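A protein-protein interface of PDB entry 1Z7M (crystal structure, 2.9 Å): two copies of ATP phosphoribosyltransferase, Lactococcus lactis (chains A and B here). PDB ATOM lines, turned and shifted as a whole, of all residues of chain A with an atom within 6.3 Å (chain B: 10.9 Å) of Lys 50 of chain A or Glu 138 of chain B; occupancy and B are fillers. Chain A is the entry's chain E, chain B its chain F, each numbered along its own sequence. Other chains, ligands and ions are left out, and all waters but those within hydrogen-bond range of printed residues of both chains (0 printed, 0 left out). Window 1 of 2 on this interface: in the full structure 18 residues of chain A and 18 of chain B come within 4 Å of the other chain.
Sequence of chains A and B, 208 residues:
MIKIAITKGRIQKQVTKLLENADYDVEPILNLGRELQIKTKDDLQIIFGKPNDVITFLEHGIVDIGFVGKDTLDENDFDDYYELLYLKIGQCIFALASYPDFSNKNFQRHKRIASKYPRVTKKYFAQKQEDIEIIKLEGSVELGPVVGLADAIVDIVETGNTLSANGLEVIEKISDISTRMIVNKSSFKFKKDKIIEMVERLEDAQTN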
ATOM      1  N   ILE A   6      11.782  19.934   1.284  1.00  0.00           N
ATOM      2  CA  ILE A   6      12.928  19.736   2.166  1.00  0.00           C
ATOM      3  C   ILE A   6      14.233  19.479   1.430  1.00  0.00           C
ATOM      4  O   ILE A   6      14.240  18.907   0.344  1.00  0.00           O
ATOM      5  CB  ILE A   6      12.702  18.548   3.111  1.00  0.00           C
ATOM      6  CG1 ILE A   6      11.268  18.576   3.648  1.00  0.00           C
ATOM      7  CG2 ILE A   6      13.704  18.610   4.265  1.00  0.00           C
ATOM      8  CD1 ILE A   6      10.887  17.376   4.492  1.00  0.00           C
ATOM      9  N   THR A   7      15.338  19.902   2.032  1.00  0.00           N
ATOM     10  CA  THR A   7      16.653  19.686   1.435  1.00  0.00           C
ATOM     11  C   THR A   7      17.060  18.218   1.650  1.00  0.00           C
ATOM     12  O   THR A   7      17.172  17.748   2.794  1.00  0.00           O
ATOM     13  CB  THR A   7      17.707  20.601   2.083  1.00  0.00           C
ATOM     14  OG1 THR A   7      17.576  20.535   3.510  1.00  0.00           O
ATOM     15  CG2 THR A   7      17.527  22.028   1.632  1.00  0.00           C
ATOM     16  N   LYS A   8      17.283  17.505   0.548  1.00  0.00           N
ATOM     17  CA  LYS A   8      17.654  16.088   0.580  1.00  0.00           C
ATOM     18  C   LYS A   8      18.850  15.737   1.458  1.00  0.00           C
ATOM     19  O   LYS A   8      19.089  14.564   1.722  1.00  0.00           O
ATOM     20  CB  LYS A   8      17.937  15.579  -0.841  1.00  0.00           C
ATOM     21  CG  LYS A   8      16.727  15.485  -1.749  1.00  0.00           C
ATOM     22  CD  LYS A   8      17.136  15.470  -3.224  1.00  0.00           C
ATOM     23  CE  LYS A   8      17.995  14.259  -3.586  1.00  0.00           C
ATOM     24  NZ  LYS A   8      18.575  14.358  -4.967  1.00  0.00           N
ATOM     25  N   PHE A  48      11.223  16.997  -2.419  1.00  0.00           N
ATOM     26  CA  PHE A  48      12.632  17.023  -1.996  1.00  0.00           C
ATOM     27  C   PHE A  48      13.573  17.495  -3.102  1.00  0.00           C
ATOM     28  O   PHE A  48      13.280  17.354  -4.293  1.00  0.00           O
ATOM     29  CB  PHE A  48      13.102  15.644  -1.516  1.00  0.00           C
ATOM     30  CG  PHE A  48      12.338  15.113  -0.345  1.00  0.00           C
ATOM     31  CD1 PHE A  48      11.061  14.591  -0.514  1.00  0.00           C
ATOM     32  CD2 PHE A  48      12.891  15.142   0.929  1.00  0.00           C
ATOM     33  CE1 PHE A  48      10.339  14.102   0.575  1.00  0.00           C
ATOM     34  CE2 PHE A  48      12.182  14.657   2.026  1.00  0.00           C
ATOM     35  CZ  PHE A  48      10.901  14.135   1.850  1.00  0.00           C
ATOM     36  N   GLY A  49      14.711  18.043  -2.690  1.00  0.00           N
ATOM     37  CA  GLY A  49      15.695  18.543  -3.632  1.00  0.00           C
ATOM     38  C   GLY A  49      16.814  19.265  -2.910  1.00  0.00           C
ATOM     39  O   GLY A  49      16.916  19.161  -1.680  1.00  0.00           O
ATOM     40  N   LYS A  50      17.639  19.995  -3.671  1.00  0.00           N
ATOM     41  CA  LYS A  50      18.786  20.749  -3.128  1.00  0.00           C
ATOM     42  C   LYS A  50      18.406  22.078  -2.478  1.00  0.00           C
ATOM     43  O   LYS A  50      17.416  22.701  -2.864  1.00  0.00           O
ATOM     44  CB  LYS A  50      19.820  21.015  -4.230  1.00  0.00           C
ATOM     45  CG  LYS A  50      20.683  19.812  -4.588  1.00  0.00           C
ATOM     46  CD  LYS A  50      21.612  20.119  -5.764  1.00  0.00           C
ATOM     47  CE  LYS A  50      22.379  18.881  -6.223  1.00  0.00           C
ATOM     48  NZ  LYS A  50      23.221  18.305  -5.131  1.00  0.00           N
ATOM     49  N   PRO A  51      19.208  22.544  -1.500  1.00  0.00           N
ATOM     50  CA  PRO A  51      18.906  23.811  -0.824  1.00  0.00           C
ATOM     51  C   PRO A  51      18.399  24.918  -1.757  1.00  0.00           C
ATOM     52  O   PRO A  51      17.250  25.340  -1.650  1.00  0.00           O
ATOM     53  N   ASN A  52      19.236  25.373  -2.683  1.00  0.00           N
ATOM     54  CA  ASN A  52      18.816  26.431  -3.594  1.00  0.00           C
ATOM     55  C   ASN A  52      17.601  26.067  -4.434  1.00  0.00           C
ATOM     56  O   ASN A  52      17.042  26.924  -5.113  1.00  0.00           O
ATOM     57  CB  ASN A  52      19.962  26.844  -4.511  1.00  0.00           C
ATOM     58  CG  ASN A  52      21.092  27.500  -3.756  1.00  0.00           C
ATOM     59  OD1 ASN A  52      20.870  28.383  -2.933  1.00  0.00           O
ATOM     60  ND2 ASN A  52      22.310  27.079  -4.039  1.00  0.00           N
ATOM     61  N   ASP A  53      17.197  24.800  -4.402  1.00  0.00           N
ATOM     62  CA  ASP A  53      16.023  24.351  -5.149  1.00  0.00           C
ATOM     63  C   ASP A  53      14.785  24.435  -4.251  1.00  0.00           C
ATOM     64  O   ASP A  53      13.685  24.732  -4.725  1.00  0.00           O
ATOM     65  CB  ASP A  53      16.243  22.925  -5.667  1.00  0.00           C
ATOM     66  CG  ASP A  53      16.565  22.897  -7.153  1.00  0.00           C
ATOM     67  OD1 ASP A  53      17.309  23.797  -7.608  1.00  0.00           O
ATOM     68  OD2 ASP A  53      16.078  21.987  -7.871  1.00  0.00           O
ATOM     69  N   VAL A  54      14.980  24.186  -2.953  1.00  0.00           N
ATOM     70  CA  VAL A  54      13.899  24.274  -1.972  1.00  0.00           C
ATOM     71  C   VAL A  54      13.436  25.717  -2.027  1.00  0.00           C
ATOM     72  O   VAL A  54      12.245  26.001  -2.133  1.00  0.00           O
ATOM     73  CB  VAL A  54      14.395  23.987  -0.534  1.00  0.00           C
ATOM     74  CG1 VAL A  54      13.346  24.411   0.469  1.00  0.00           C
ATOM     75  CG2 VAL A  54      14.696  22.522  -0.364  1.00  0.00           C
ATOM     76  N   ILE A  55      14.406  26.621  -1.947  1.00  0.00           N
ATOM     77  CA  ILE A  55      14.149  28.047  -2.015  1.00  0.00           C
ATOM     78  C   ILE A  55      13.474  28.392  -3.336  1.00  0.00           C
ATOM     79  O   ILE A  55      12.449  29.061  -3.341  1.00  0.00           O
ATOM     80  CB  ILE A  55      15.450  28.847  -1.863  1.00  0.00           C
ATOM     81  CG1 ILE A  55      15.877  28.811  -0.390  1.00  0.00           C
ATOM     82  CG2 ILE A  55      15.269  30.260  -2.389  1.00  0.00           C
ATOM     83  CD1 ILE A  55      17.216  29.452  -0.085  1.00  0.00           C
ATOM     84  N   VAL A  68      15.510  24.592   5.093  1.00  0.00           N
ATOM     85  CA  VAL A  68      16.856  24.779   4.575  1.00  0.00           C
ATOM     86  C   VAL A  68      17.780  25.232   5.689  1.00  0.00           C
ATOM     87  O   VAL A  68      17.387  25.297   6.852  1.00  0.00           O
ATOM     88  CB  VAL A  68      16.887  25.827   3.463  1.00  0.00           C
ATOM     89  CG1 VAL A  68      16.543  25.187   2.142  1.00  0.00           C
ATOM     90  CG2 VAL A  68      15.893  26.919   3.769  1.00  0.00           C
ATOM     91  N   LYS B  50      34.768  18.948  -8.376  1.00  0.00           N
ATOM     92  CA  LYS B  50      33.641  19.097  -9.270  1.00  0.00           C
ATOM     93  C   LYS B  50      34.101  19.627 -10.640  1.00  0.00           C
ATOM     94  O   LYS B  50      35.208  20.144 -10.777  1.00  0.00           O
ATOM     95  CB  LYS B  50      32.607  20.006  -8.615  1.00  0.00           C
ATOM     96  CG  LYS B  50      32.037  19.412  -7.330  1.00  0.00           C
ATOM     97  CD  LYS B  50      30.610  19.883  -7.110  1.00  0.00           C
ATOM     98  CE  LYS B  50      29.920  19.121  -6.006  1.00  0.00           C
ATOM     99  NZ  LYS B  50      28.501  19.554  -5.919  1.00  0.00           N
ATOM    100  N   PRO B  51      33.243  19.521 -11.669  1.00  0.00           N
ATOM    101  CA  PRO B  51      33.571  19.973 -13.029  1.00  0.00           C
ATOM    102  C   PRO B  51      34.116  21.375 -13.087  1.00  0.00           C
ATOM    103  O   PRO B  51      35.226  21.606 -13.568  1.00  0.00           O
ATOM    104  CB  PRO B  51      32.238  19.879 -13.755  1.00  0.00           C
ATOM    105  CG  PRO B  51      31.287  20.286 -12.676  1.00  0.00           C
ATOM    106  CD  PRO B  51      31.779  19.451 -11.505  1.00  0.00           C
ATOM    107  N   ASN B  52      33.298  22.302 -12.601  1.00  0.00           N
ATOM    108  CA  ASN B  52      33.601  23.727 -12.558  1.00  0.00           C
ATOM    109  C   ASN B  52      34.873  24.009 -11.762  1.00  0.00           C
ATOM    110  O   ASN B  52      35.630  24.931 -12.081  1.00  0.00           O
ATOM    111  CB  ASN B  52      32.403  24.457 -11.962  1.00  0.00           C
ATOM    112  CG  ASN B  52      31.127  24.178 -12.730  1.00  0.00           C
ATOM    113  OD1 ASN B  52      30.853  24.813 -13.753  1.00  0.00           O
ATOM    114  ND2 ASN B  52      30.349  23.203 -12.256  1.00  0.00           N
ATOM    115  N   ASP B  71      29.295  18.887 -21.550  1.00  0.00           N
ATOM    116  CA  ASP B  71      28.211  19.709 -21.018  1.00  0.00           C
ATOM    117  C   ASP B  71      28.800  20.893 -20.240  1.00  0.00           C
ATOM    118  O   ASP B  71      28.547  22.062 -20.575  1.00  0.00           O
ATOM    119  CB  ASP B  71      27.292  18.869 -20.125  1.00  0.00           C
ATOM    120  CG  ASP B  71      28.029  18.211 -18.998  1.00  0.00           C
ATOM    121  OD1 ASP B  71      29.000  17.477 -19.270  1.00  0.00           O
ATOM    122  OD2 ASP B  71      27.642  18.426 -17.835  1.00  0.00           O
ATOM    123  N   ILE B 113      11.421  27.455 -19.165  1.00  0.00           N
ATOM    124  CA  ILE B 113      12.171  26.205 -19.140  1.00  0.00           C
ATOM    125  C   ILE B 113      13.072  26.134 -17.917  1.00  0.00           C
ATOM    126  O   ILE B 113      13.773  27.088 -17.605  1.00  0.00           O
ATOM    127  CB  ILE B 113      13.069  26.060 -20.386  1.00  0.00           C
ATOM    128  CG1 ILE B 113      12.223  26.070 -21.660  1.00  0.00           C
ATOM    129  CG2 ILE B 113      13.876  24.774 -20.298  1.00  0.00           C
ATOM    130  CD1 ILE B 113      11.757  27.444 -22.084  1.00  0.00           C
ATOM    131  N   ALA B 114      13.060  25.002 -17.228  1.00  0.00           N
ATOM    132  CA  ALA B 114      13.909  24.830 -16.054  1.00  0.00           C
ATOM    133  C   ALA B 114      15.063  23.874 -16.370  1.00  0.00           C
ATOM    134  O   ALA B 114      14.837  22.738 -16.795  1.00  0.00           O
ATOM    135  CB  ALA B 114      13.089  24.292 -14.884  1.00  0.00           C
ATOM    136  N   SER B 115      16.294  24.329 -16.155  1.00  0.00           N
ATOM    137  CA  SER B 115      17.457  23.499 -16.422  1.00  0.00           C
ATOM    138  C   SER B 115      18.582  23.787 -15.449  1.00  0.00           C
ATOM    139  O   SER B 115      18.495  24.705 -14.642  1.00  0.00           O
ATOM    140  CB  SER B 115      17.955  23.730 -17.846  1.00  0.00           C
ATOM    141  OG  SER B 115      18.386  25.058 -18.028  1.00  0.00           O
ATOM    142  N   LYS B 116      19.635  22.983 -15.530  1.00  0.00           N
ATOM    143  CA  LYS B 116      20.800  23.141 -14.672  1.00  0.00           C
ATOM    144  C   LYS B 116      21.871  23.829 -15.523  1.00  0.00           C
ATOM    145  O   LYS B 116      22.935  24.217 -15.033  1.00  0.00           O
ATOM    146  CB  LYS B 116      21.284  21.763 -14.208  1.00  0.00           C
ATOM    147  CG  LYS B 116      22.375  21.781 -13.152  1.00  0.00           C
ATOM    148  CD  LYS B 116      22.965  20.384 -12.924  1.00  0.00           C
ATOM    149  CE  LYS B 116      23.982  20.378 -11.769  1.00  0.00           C
ATOM    150  NZ  LYS B 116      24.774  19.100 -11.680  1.00  0.00           N
ATOM    151  N   TYR B 117      21.567  23.969 -16.812  1.00  0.00           N
ATOM    152  CA  TYR B 117      22.476  24.589 -17.773  1.00  0.00           C
ATOM    153  C   TYR B 117      21.792  25.797 -18.405  1.00  0.00           C
ATOM    154  O   TYR B 117      21.456  25.780 -19.595  1.00  0.00           O
ATOM    155  CB  TYR B 117      22.879  23.586 -18.885  1.00  0.00           C
ATOM    156  CG  TYR B 117      23.451  22.274 -18.365  1.00  0.00           C
ATOM    157  CD1 TYR B 117      22.606  21.271 -17.867  1.00  0.00           C
ATOM    158  CD2 TYR B 117      24.837  22.081 -18.257  1.00  0.00           C
ATOM    159  CE1 TYR B 117      23.123  20.118 -17.259  1.00  0.00           C
ATOM    160  CE2 TYR B 117      25.361  20.924 -17.649  1.00  0.00           C
ATOM    161  CZ  TYR B 117      24.498  19.958 -17.148  1.00  0.00           C
ATOM    162  OH  TYR B 117      25.002  18.858 -16.493  1.00  0.00           O
ATOM    163  N   PRO B 118      21.575  26.863 -17.616  1.00  0.00           N
ATOM    164  CA  PRO B 118      20.921  28.074 -18.124  1.00  0.00           C
ATOM    165  C   PRO B 118      21.608  28.736 -19.313  1.00  0.00           C
ATOM    166  O   PRO B 118      20.952  29.223 -20.232  1.00  0.00           O
ATOM    167  CB  PRO B 118      20.858  28.978 -16.891  1.00  0.00           C
ATOM    168  CG  PRO B 118      21.993  28.513 -16.068  1.00  0.00           C
ATOM    169  CD  PRO B 118      21.917  27.017 -16.195  1.00  0.00           C
ATOM    170  N   ILE B 134      14.225  31.353 -18.131  1.00  0.00           N
ATOM    171  CA  ILE B 134      14.926  30.238 -17.509  1.00  0.00           C
ATOM    172  C   ILE B 134      14.748  30.160 -15.993  1.00  0.00           C
ATOM    173  O   ILE B 134      14.837  31.170 -15.306  1.00  0.00           O
ATOM    174  CB  ILE B 134      16.439  30.325 -17.787  1.00  0.00           C
ATOM    175  CG1 ILE B 134      16.709  30.373 -19.294  1.00  0.00           C
ATOM    176  CG2 ILE B 134      17.141  29.153 -17.147  1.00  0.00           C
ATOM    177  CD1 ILE B 134      16.411  31.701 -19.945  1.00  0.00           C
ATOM    178  N   ILE B 135      14.510  28.964 -15.467  1.00  0.00           N
ATOM    179  CA  ILE B 135      14.355  28.784 -14.021  1.00  0.00           C
ATOM    180  C   ILE B 135      15.446  27.840 -13.519  1.00  0.00           C
ATOM    181  O   ILE B 135      15.298  26.621 -13.570  1.00  0.00           O
ATOM    182  CB  ILE B 135      12.980  28.168 -13.661  1.00  0.00           C
ATOM    183  CG1 ILE B 135      11.851  29.079 -14.149  1.00  0.00           C
ATOM    184  CG2 ILE B 135      12.891  27.902 -12.161  1.00  0.00           C
ATOM    185  CD1 ILE B 135      11.956  30.524 -13.669  1.00  0.00           C
ATOM    186  N   LYS B 136      16.536  28.410 -13.021  1.00  0.00           N
ATOM    187  CA  LYS B 136      17.656  27.618 -12.530  1.00  0.00           C
ATOM    188  C   LYS B 136      17.318  26.564 -11.464  1.00  0.00           C
ATOM    189  O   LYS B 136      16.743  26.861 -10.405  1.00  0.00           O
ATOM    190  CB  LYS B 136      18.766  28.543 -12.002  1.00  0.00           C
ATOM    191  CG  LYS B 136      19.258  29.583 -13.024  1.00  0.00           C
ATOM    192  CD  LYS B 136      20.456  30.419 -12.514  1.00  0.00           C
ATOM    193  CE  LYS B 136      21.025  31.356 -13.607  1.00  0.00           C
ATOM    194  NZ  LYS B 136      22.289  32.072 -13.201  1.00  0.00           N
ATOM    195  N   LEU B 137      17.674  25.319 -11.769  1.00  0.00           N
ATOM    196  CA  LEU B 137      17.474  24.204 -10.860  1.00  0.00           C
ATOM    197  C   LEU B 137      18.770  23.451 -10.789  1.00  0.00           C
ATOM    198  O   LEU B 137      19.413  23.204 -11.804  1.00  0.00           O
ATOM    199  CB  LEU B 137      16.382  23.267 -11.360  1.00  0.00           C
ATOM    200  CG  LEU B 137      14.973  23.779 -11.114  1.00  0.00           C
ATOM    201  CD1 LEU B 137      13.981  22.741 -11.587  1.00  0.00           C
ATOM    202  CD2 LEU B 137      14.792  24.069  -9.632  1.00  0.00           C
ATOM    203  N   GLU B 138      19.166  23.097  -9.583  1.00  0.00           N
ATOM    204  CA  GLU B 138      20.386  22.349  -9.398  1.00  0.00           C
ATOM    205  C   GLU B 138      20.076  20.855  -9.503  1.00  0.00           C
ATOM    206  O   GLU B 138      20.979  20.024  -9.599  1.00  0.00           O
ATOM    207  CB  GLU B 138      20.985  22.682  -8.036  1.00  0.00           C
ATOM    208  CG  GLU B 138      21.490  24.107  -7.932  1.00  0.00           C
ATOM    209  CD  GLU B 138      22.007  24.437  -6.550  1.00  0.00           C
ATOM    210  OE1 GLU B 138      22.834  25.367  -6.451  1.00  0.00           O
ATOM    211  OE2 GLU B 138      21.581  23.788  -5.559  1.00  0.00           O
ATOM    212  N   SER B 140      17.422  17.641  -9.942  1.00  0.00           N
ATOM    213  CA  SER B 140      16.297  16.821 -10.405  1.00  0.00           C
ATOM    214  C   SER B 140      15.395  17.649 -11.314  1.00  0.00           C
ATOM    215  O   SER B 140      14.191  17.762 -11.090  1.00  0.00           O
ATOM    216  CB  SER B 140      15.479  16.308  -9.213  1.00  0.00           C
ATOM    217  OG  SER B 140      16.290  15.588  -8.297  1.00  0.00           O
ATOM    218  N   VAL B 141      15.995  18.214 -12.352  1.00  0.00           N
ATOM    219  CA  VAL B 141      15.291  19.069 -13.298  1.00  0.00           C
ATOM    220  C   VAL B 141      13.933  18.569 -13.795  1.00  0.00           C
ATOM    221  O   VAL B 141      13.151  19.349 -14.346  1.00  0.00           O
ATOM    222  CB  VAL B 141      16.195  19.378 -14.529  1.00  0.00           C
ATOM    223  CG1 VAL B 141      15.601  20.523 -15.336  1.00  0.00           C
ATOM    224  CG2 VAL B 141      17.607  19.731 -14.066  1.00  0.00           C
ATOM    225  N   GLU B 142      13.643  17.285 -13.599  1.00  0.00           N
ATOM    226  CA  GLU B 142      12.367  16.711 -14.053  1.00  0.00           C
ATOM    227  C   GLU B 142      11.121  17.358 -13.403  1.00  0.00           C
ATOM    228  O   GLU B 142      10.116  17.606 -14.089  1.00  0.00           O
ATOM    229  CB  GLU B 142      12.344  15.196 -13.801  1.00  0.00           C
ATOM    230  CG  GLU B 142      13.544  14.437 -14.350  1.00  0.00           C
ATOM    231  CD  GLU B 142      14.733  14.448 -13.404  1.00  0.00           C
ATOM    232  OE1 GLU B 142      14.547  14.091 -12.220  1.00  0.00           O
ATOM    233  OE2 GLU B 142      15.853  14.798 -13.841  1.00  0.00           O
ATOM    234  N   LEU B 143      11.196  17.633 -12.094  1.00  0.00           N
ATOM    235  CA  LEU B 143      10.084  18.240 -11.350  1.00  0.00           C
ATOM    236  C   LEU B 143       9.655  19.582 -11.901  1.00  0.00           C
ATOM    237  O   LEU B 143       8.565  20.048 -11.596  1.00  0.00           O
ATOM    238  CB  LEU B 143      10.432  18.426  -9.868  1.00  0.00           C
ATOM    239  CG  LEU B 143      10.602  17.184  -8.998  1.00  0.00           C
ATOM    240  CD1 LEU B 143      11.845  16.437  -9.450  1.00  0.00           C
ATOM    241  CD2 LEU B 143      10.724  17.589  -7.530  1.00  0.00           C
ATOM    242  N   GLY B 144      10.516  20.202 -12.701  1.00  0.00           N
ATOM    243  CA  GLY B 144      10.199  21.499 -13.276  1.00  0.00           C
ATOM    244  C   GLY B 144       8.786  21.556 -13.816  1.00  0.00           C
ATOM    245  O   GLY B 144       7.976  22.382 -13.386  1.00  0.00           O
ATOM    246  N   LEU B 149       6.098  24.141 -12.081  1.00  0.00           N
ATOM    247  CA  LEU B 149       7.105  25.191 -11.910  1.00  0.00           C
ATOM    248  C   LEU B 149       7.659  25.759 -13.215  1.00  0.00           C
ATOM    249  O   LEU B 149       8.095  26.916 -13.264  1.00  0.00           O
ATOM    250  CB  LEU B 149       8.271  24.660 -11.076  1.00  0.00           C
ATOM    251  CG  LEU B 149       9.450  25.627 -10.977  1.00  0.00           C
ATOM    252  CD1 LEU B 149       9.028  26.821 -10.139  1.00  0.00           C
ATOM    253  CD2 LEU B 149      10.670  24.928 -10.372  1.00  0.00           C
ATOM    254  N   ILE B 153      11.987  21.227 -20.083  1.00  0.00           N
ATOM    255  CA  ILE B 153      13.319  21.380 -19.519  1.00  0.00           C
ATOM    256  C   ILE B 153      14.450  21.105 -20.515  1.00  0.00           C
ATOM    257  O   ILE B 153      14.270  20.406 -21.515  1.00  0.00           O
ATOM    258  CB  ILE B 153      13.495  20.463 -18.315  1.00  0.00           C
ATOM    259  CG1 ILE B 153      13.532  19.007 -18.772  1.00  0.00           C
ATOM    260  CG2 ILE B 153      12.353  20.680 -17.349  1.00  0.00           C
ATOM    261  CD1 ILE B 153      13.841  18.022 -17.670  1.00  0.00           C
ATOM    262  N   VAL B 154      15.620  21.674 -20.239  1.00  0.00           N
ATOM    263  CA  VAL B 154      16.793  21.474 -21.080  1.00  0.00           C
ATOM    264  C   VAL B 154      17.865  20.816 -20.203  1.00  0.00           C
ATOM    265  O   VAL B 154      18.731  21.480 -19.627  1.00  0.00           O
ATOM    266  CB  VAL B 154      17.298  22.818 -21.660  1.00  0.00           C
ATOM    267  CG1 VAL B 154      18.527  22.591 -22.503  1.00  0.00           C
ATOM    268  CG2 VAL B 154      16.207  23.461 -22.503  1.00  0.00           C
ATOM    269  N   ASP B 155      17.778  19.493 -20.099  1.00  0.00           N
ATOM    270  CA  ASP B 155      18.705  18.715 -19.294  1.00  0.00           C
ATOM    271  C   ASP B 155      19.483  17.693 -20.125  1.00  0.00           C
ATOM    272  O   ASP B 155      19.335  17.615 -21.341  1.00  0.00           O
ATOM    273  CB  ASP B 155      17.938  17.992 -18.189  1.00  0.00           C
ATOM    274  CG  ASP B 155      18.795  17.710 -16.971  1.00  0.00           C
ATOM    275  OD1 ASP B 155      18.343  16.942 -16.098  1.00  0.00           O
ATOM    276  OD2 ASP B 155      19.911  18.264 -16.870  1.00  0.00           O
ATOM    277  N   ILE B 156      20.327  16.922 -19.452  1.00  0.00           N
ATOM    278  CA  ILE B 156      21.114  15.890 -20.109  1.00  0.00           C
ATOM    279  C   ILE B 156      20.317  14.584 -20.050  1.00  0.00           C
ATOM    280  O   ILE B 156      20.040  14.053 -18.964  1.00  0.00           O
ATOM    281  CB  ILE B 156      22.508  15.695 -19.419  1.00  0.00           C
ATOM    282  CG1 ILE B 156      22.336  15.530 -17.908  1.00  0.00           C
ATOM    283  CG2 ILE B 156      23.409  16.883 -19.705  1.00  0.00           C
ATOM    284  CD1 ILE B 156      23.641  15.547 -17.144  1.00  0.00           C
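The backbone carbonyl oxygen of Ser 115 of chain B is in hydrogen-bond range of the backbone NH of Leu 137 of chain B, 3.1 Å away.
No residue of chain B comes within 4 Å of Thr 7 of chain A.
No residue of chain B comes within 4 Å of Gly 49 of chain A.
No residue of chain B comes within 4 Å of Pro 51 of chain A.
Printed residues of chain B within 4 Å of Asn 52 of chain A: Glu 138.
Printed residues of chain A within 4 Å of Leu 137 of chain B: Asp 53 (3.0 Å).
The nearest residue of chain A that does not touch Glu 138 of chain B is Pro 51 of chain A (4.9 Å).
The nearest printed residue of chain A that does not touch Leu 137 of chain B is Asn 52 of chain A (5.8 Å).
The backbone NH (N) of Glu 138 of chain B lies within hydrogen-bond range of the side-chain carboxylate (OD1) of Asp 53 of chain A (2.8 Å).
The side-chain amide nitrogen (ND2) of Asn 52 of chain A sits at hydrogen-bond distance from the side-chain carboxylate (OE1) of Glu 138 of chain B, at 3.0 Å.
CB of Glu 138 of chain B touches CD of Lys 50 of chain A, 3.5 Å away.
CD2 of Leu 137 of chain B touches OD2 of Asp 53 of chain A, 3.0 Å away.
Printed residues of chain B that touch a printed residue of chain A: Leu 137 and Glu 138.
Hydrophobic or aromatic side chains of chain B that line the printed part of chain A: Leu 137.
Among the printed residues, 4 pairs touch across the chains.
Among the printed residues, no Asp or Glu carboxylate lies within 4 Å of a Lys or Arg side-chain nitrogen of the other chain.
3 positions are printed for both chains.
Of the 4 pairs that touch across the chains among the printed residues, none has its exchanged pair printed and touching as well.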
